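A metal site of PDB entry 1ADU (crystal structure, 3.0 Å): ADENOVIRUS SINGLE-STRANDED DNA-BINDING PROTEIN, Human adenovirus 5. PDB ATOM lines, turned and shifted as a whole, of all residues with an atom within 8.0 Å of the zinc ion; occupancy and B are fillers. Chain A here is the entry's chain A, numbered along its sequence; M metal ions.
The zinc ion is bound by ND1 of His 113 (2.0 Å), SG of Cys 166 (2.3 Å), SG of Cys 182 (2.3 Å) and SG of Cys 111 (2.3 Å).
Within 4 Å of the zinc ion: Cys 111, His 113, Cys 166 and Cys 182.
The side-chain hydroxyl (OG) of Ser 115 sits close to the side-chain sulfur (SG) of Cys 111 (3.5 Å). The indole nitrogen (NE1) of Trp 331 sits close to a ring nitrogen (NE2) of His 113 (3.3 Å). The side-chain sulfur (SG) of Cys 166 lies close to the backbone NH (N) of His 168. N of Cys 111 lies within hydrogen-bond range of SD of Met 117, at 3.5 Å. The side-chain sulfur of Cys 182 lies close to the backbone NH of Met 184 (3.6 Å).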
ATOM      1  N   LYS A 110     -15.770 -11.200  12.157  1.00  0.00           N
ATOM      2  CA  LYS A 110     -14.574 -12.023  12.206  1.00  0.00           C
ATOM      3  C   LYS A 110     -14.934 -13.429  12.651  1.00  0.00           C
ATOM      4  O   LYS A 110     -15.468 -13.602  13.745  1.00  0.00           O
ATOM      5  CB  LYS A 110     -13.552 -11.431  13.176  1.00  0.00           C
ATOM      6  CG  LYS A 110     -12.903 -10.136  12.731  1.00  0.00           C
ATOM      7  CD  LYS A 110     -11.807  -9.751  13.711  1.00  0.00           C
ATOM      8  CE  LYS A 110     -10.794  -8.804  13.098  1.00  0.00           C
ATOM      9  NZ  LYS A 110      -9.418  -9.081  13.602  1.00  0.00           N
ATOM     10  N   CYS A 111     -14.673 -14.426  11.809  1.00  0.00           N
ATOM     11  CA  CYS A 111     -14.977 -15.819  12.139  1.00  0.00           C
ATOM     12  C   CYS A 111     -14.129 -16.320  13.302  1.00  0.00           C
ATOM     13  O   CYS A 111     -13.223 -15.618  13.754  1.00  0.00           O
ATOM     14  CB  CYS A 111     -14.758 -16.718  10.921  1.00  0.00           C
ATOM     15  SG  CYS A 111     -13.014 -16.980  10.436  1.00  0.00           S
ATOM     16  N   LEU A 112     -14.375 -17.548  13.745  1.00  0.00           N
ATOM     17  CA  LEU A 112     -13.625 -18.150  14.858  1.00  0.00           C
ATOM     18  C   LEU A 112     -12.114 -18.247  14.659  1.00  0.00           C
ATOM     19  O   LEU A 112     -11.409 -18.772  15.509  1.00  0.00           O
ATOM     20  CB  LEU A 112     -14.156 -19.556  15.146  1.00  0.00           C
ATOM     21  CG  LEU A 112     -15.609 -19.712  15.558  1.00  0.00           C
ATOM     22  CD1 LEU A 112     -15.919 -21.195  15.670  1.00  0.00           C
ATOM     23  CD2 LEU A 112     -15.862 -19.000  16.864  1.00  0.00           C
ATOM     24  N   HIS A 113     -11.636 -17.802  13.495  1.00  0.00           N
ATOM     25  CA  HIS A 113     -10.211 -17.861  13.190  1.00  0.00           C
ATOM     26  C   HIS A 113      -9.490 -16.609  13.653  1.00  0.00           C
ATOM     27  O   HIS A 113      -8.281 -16.618  13.856  1.00  0.00           O
ATOM     28  CB  HIS A 113      -9.994 -18.044  11.694  1.00  0.00           C
ATOM     29  CG  HIS A 113     -10.126 -19.454  11.229  1.00  0.00           C
ATOM     30  ND1 HIS A 113     -11.138 -19.834  10.391  1.00  0.00           N
ATOM     31  CD2 HIS A 113      -9.319 -20.524  11.471  1.00  0.00           C
ATOM     32  CE1 HIS A 113     -10.934 -21.113  10.127  1.00  0.00           C
ATOM     33  NE2 HIS A 113      -9.846 -21.572  10.760  1.00  0.00           N
ATOM     34  N   GLY A 114     -10.252 -15.529  13.827  1.00  0.00           N
ATOM     35  CA  GLY A 114      -9.666 -14.262  14.235  1.00  0.00           C
ATOM     36  C   GLY A 114      -9.410 -13.435  13.005  1.00  0.00           C
ATOM     37  O   GLY A 114      -8.861 -12.334  13.082  1.00  0.00           O
ATOM     38  N   SER A 115      -9.828 -13.956  11.860  1.00  0.00           N
ATOM     39  CA  SER A 115      -9.659 -13.294  10.579  1.00  0.00           C
ATOM     40  C   SER A 115     -10.967 -12.708  10.068  1.00  0.00           C
ATOM     41  O   SER A 115     -12.041 -13.206  10.399  1.00  0.00           O
ATOM     42  CB  SER A 115      -9.129 -14.302   9.548  1.00  0.00           C
ATOM     43  OG  SER A 115     -10.005 -15.404   9.413  1.00  0.00           O
ATOM     44  N   ILE A 116     -10.864 -11.680   9.232  1.00  0.00           N
ATOM     45  CA  ILE A 116     -12.054 -11.052   8.669  1.00  0.00           C
ATOM     46  C   ILE A 116     -12.918 -12.050   7.907  1.00  0.00           C
ATOM     47  O   ILE A 116     -12.562 -13.224   7.790  1.00  0.00           O
ATOM     48  CB  ILE A 116     -11.698  -9.860   7.722  1.00  0.00           C
ATOM     49  CG1 ILE A 116     -10.427 -10.162   6.929  1.00  0.00           C
ATOM     50  CG2 ILE A 116     -11.561  -8.557   8.531  1.00  0.00           C
ATOM     51  CD1 ILE A 116      -9.972  -9.032   6.024  1.00  0.00           C
ATOM     52  N   MET A 117     -14.071 -11.603   7.425  1.00  0.00           N
ATOM     53  CA  MET A 117     -14.966 -12.481   6.694  1.00  0.00           C
ATOM     54  C   MET A 117     -15.259 -11.944   5.307  1.00  0.00           C
ATOM     55  O   MET A 117     -15.522 -10.757   5.107  1.00  0.00           O
ATOM     56  CB  MET A 117     -16.253 -12.762   7.486  1.00  0.00           C
ATOM     57  CG  MET A 117     -16.044 -13.835   8.569  1.00  0.00           C
ATOM     58  SD  MET A 117     -17.432 -14.183   9.682  1.00  0.00           S
ATOM     59  CE  MET A 117     -18.245 -15.517   8.851  1.00  0.00           C
ATOM     60  N   CYS A 165     -18.615 -15.078   5.014  1.00  0.00           N
ATOM     61  CA  CYS A 165     -18.154 -16.430   5.225  1.00  0.00           C
ATOM     62  C   CYS A 165     -16.705 -16.427   5.650  1.00  0.00           C
ATOM     63  O   CYS A 165     -16.003 -15.426   5.494  1.00  0.00           O
ATOM     64  CB  CYS A 165     -18.308 -17.243   3.948  1.00  0.00           C
ATOM     65  SG  CYS A 165     -17.314 -16.615   2.584  1.00  0.00           S
ATOM     66  N   CYS A 166     -16.282 -17.539   6.232  1.00  0.00           N
ATOM     67  CA  CYS A 166     -14.907 -17.715   6.670  1.00  0.00           C
ATOM     68  C   CYS A 166     -13.952 -17.593   5.471  1.00  0.00           C
ATOM     69  O   CYS A 166     -14.223 -18.150   4.402  1.00  0.00           O
ATOM     70  CB  CYS A 166     -14.802 -19.091   7.331  1.00  0.00           C
ATOM     71  SG  CYS A 166     -13.119 -19.647   7.665  1.00  0.00           S
ATOM     72  N   VAL A 167     -12.839 -16.891   5.651  1.00  0.00           N
ATOM     73  CA  VAL A 167     -11.866 -16.686   4.563  1.00  0.00           C
ATOM     74  C   VAL A 167     -11.406 -17.980   3.888  1.00  0.00           C
ATOM     75  O   VAL A 167     -11.143 -18.011   2.695  1.00  0.00           O
ATOM     76  CB  VAL A 167     -10.615 -15.873   5.025  1.00  0.00           C
ATOM     77  CG1 VAL A 167      -9.678 -16.743   5.872  1.00  0.00           C
ATOM     78  CG2 VAL A 167      -9.883 -15.294   3.827  1.00  0.00           C
ATOM     79  N   HIS A 168     -11.341 -19.065   4.666  1.00  0.00           N
ATOM     80  CA  HIS A 168     -10.917 -20.352   4.130  1.00  0.00           C
ATOM     81  C   HIS A 168     -12.018 -21.031   3.319  1.00  0.00           C
ATOM     82  O   HIS A 168     -11.921 -22.219   3.007  1.00  0.00           O
ATOM     83  CB  HIS A 168     -10.435 -21.264   5.260  1.00  0.00           C
ATOM     84  CG  HIS A 168      -9.327 -20.657   6.054  1.00  0.00           C
ATOM     85  ND1 HIS A 168      -7.995 -20.885   5.767  1.00  0.00           N
ATOM     86  CD2 HIS A 168      -9.334 -19.795   7.098  1.00  0.00           C
ATOM     87  CE1 HIS A 168      -7.240 -20.191   6.596  1.00  0.00           C
ATOM     88  NE2 HIS A 168      -8.032 -19.522   7.423  1.00  0.00           N
ATOM     89  N   ASP A 169     -13.078 -20.296   3.016  1.00  0.00           N
ATOM     90  CA  ASP A 169     -14.176 -20.791   2.207  1.00  0.00           C
ATOM     91  C   ASP A 169     -14.285 -19.868   0.998  1.00  0.00           C
ATOM     92  O   ASP A 169     -15.329 -19.795   0.358  1.00  0.00           O
ATOM     93  CB  ASP A 169     -15.496 -20.795   2.981  1.00  0.00           C
ATOM     94  CG  ASP A 169     -15.540 -21.849   4.084  1.00  0.00           C
ATOM     95  OD1 ASP A 169     -14.942 -22.927   3.909  1.00  0.00           O
ATOM     96  OD2 ASP A 169     -16.179 -21.593   5.118  1.00  0.00           O
ATOM     97  N   LYS A 180     -10.947 -26.627   5.895  1.00  0.00           N
ATOM     98  CA  LYS A 180     -10.153 -25.764   6.771  1.00  0.00           C
ATOM     99  C   LYS A 180     -11.080 -24.730   7.433  1.00  0.00           C
ATOM    100  O   LYS A 180     -10.622 -23.826   8.146  1.00  0.00           O
ATOM    101  CB  LYS A 180      -9.068 -25.048   5.968  1.00  0.00           C
ATOM    102  CG  LYS A 180      -8.176 -25.951   5.132  1.00  0.00           C
ATOM    103  CD  LYS A 180      -7.096 -26.624   5.967  1.00  0.00           C
ATOM    104  CE  LYS A 180      -5.969 -25.644   6.311  1.00  0.00           C
ATOM    105  NZ  LYS A 180      -5.348 -25.046   5.097  1.00  0.00           N
ATOM    106  N   SER A 181     -12.376 -24.849   7.158  1.00  0.00           N
ATOM    107  CA  SER A 181     -13.362 -23.929   7.681  1.00  0.00           C
ATOM    108  C   SER A 181     -13.623 -24.070   9.172  1.00  0.00           C
ATOM    109  O   SER A 181     -13.271 -25.075   9.809  1.00  0.00           O
ATOM    110  CB  SER A 181     -14.691 -24.096   6.932  1.00  0.00           C
ATOM    111  OG  SER A 181     -15.628 -23.084   7.293  1.00  0.00           O
ATOM    112  N   CYS A 182     -14.232 -23.025   9.728  1.00  0.00           N
ATOM    113  CA  CYS A 182     -14.592 -22.995  11.140  1.00  0.00           C
ATOM    114  C   CYS A 182     -16.107 -23.227  11.180  1.00  0.00           C
ATOM    115  O   CYS A 182     -16.706 -23.359  12.249  1.00  0.00           O
ATOM    116  CB  CYS A 182     -14.223 -21.643  11.738  1.00  0.00           C
ATOM    117  SG  CYS A 182     -14.838 -20.228  10.769  1.00  0.00           S
ATOM    118  N   GLY A 183     -16.717 -23.284  10.005  1.00  0.00           N
ATOM    119  CA  GLY A 183     -18.137 -23.523   9.904  1.00  0.00           C
ATOM    120  C   GLY A 183     -18.971 -22.266  10.024  1.00  0.00           C
ATOM    121  O   GLY A 183     -20.189 -22.319   9.902  1.00  0.00           O
ATOM    122  N   MET A 184     -18.326 -21.129  10.225  1.00  0.00           N
ATOM    123  CA  MET A 184     -19.074 -19.890  10.366  1.00  0.00           C
ATOM    124  C   MET A 184     -19.545 -19.313   9.035  1.00  0.00           C
ATOM    125  O   MET A 184     -18.790 -19.238   8.078  1.00  0.00           O
ATOM    126  CB  MET A 184     -18.261 -18.853  11.146  1.00  0.00           C
ATOM    127  CG  MET A 184     -19.128 -17.958  12.027  1.00  0.00           C
ATOM    128  SD  MET A 184     -18.395 -17.552  13.622  1.00  0.00           S
ATOM    129  CE  MET A 184     -18.326 -15.740  13.497  1.00  0.00           C
ATOM    130  N   PHE A 185     -20.824 -18.932   9.000  1.00  0.00           N
ATOM    131  CA  PHE A 185     -21.438 -18.332   7.814  1.00  0.00           C
ATOM    132  C   PHE A 185     -22.657 -17.510   8.239  1.00  0.00           C
ATOM    133  O   PHE A 185     -23.423 -17.931   9.114  1.00  0.00           O
ATOM    134  CB  PHE A 185     -21.871 -19.418   6.810  1.00  0.00           C
ATOM    135  CG  PHE A 185     -22.609 -18.874   5.617  1.00  0.00           C
ATOM    136  CD1 PHE A 185     -21.916 -18.465   4.492  1.00  0.00           C
ATOM    137  CD2 PHE A 185     -23.985 -18.721   5.640  1.00  0.00           C
ATOM    138  CE1 PHE A 185     -22.584 -17.903   3.406  1.00  0.00           C
ATOM    139  CE2 PHE A 185     -24.659 -18.168   4.566  1.00  0.00           C
ATOM    140  CZ  PHE A 185     -23.962 -17.751   3.443  1.00  0.00           C
ATOM    141  N   TRP A 331      -8.448 -20.883  18.679  1.00  0.00           N
ATOM    142  CA  TRP A 331      -8.674 -21.748  17.521  1.00  0.00           C
ATOM    143  C   TRP A 331      -7.671 -22.872  17.416  1.00  0.00           C
ATOM    144  O   TRP A 331      -6.484 -22.701  17.691  1.00  0.00           O
ATOM    145  CB  TRP A 331      -8.660 -20.947  16.225  1.00  0.00           C
ATOM    146  CG  TRP A 331      -8.817 -21.825  15.023  1.00  0.00           C
ATOM    147  CD1 TRP A 331      -7.829 -22.235  14.177  1.00  0.00           C
ATOM    148  CD2 TRP A 331     -10.014 -22.474  14.582  1.00  0.00           C
ATOM    149  NE1 TRP A 331      -8.333 -23.113  13.255  1.00  0.00           N
ATOM    150  CE2 TRP A 331      -9.673 -23.281  13.472  1.00  0.00           C
ATOM    151  CE3 TRP A 331     -11.343 -22.474  15.028  1.00  0.00           C
ATOM    152  CZ2 TRP A 331     -10.615 -24.067  12.798  1.00  0.00           C
ATOM    153  CZ3 TRP A 331     -12.280 -23.251  14.355  1.00  0.00           C
ATOM    154  CH2 TRP A 331     -11.906 -24.044  13.256  1.00  0.00           C
HETATM  155 ZN    ZN M   1     -12.967 -19.234   9.903  1.00  0.00          ZN
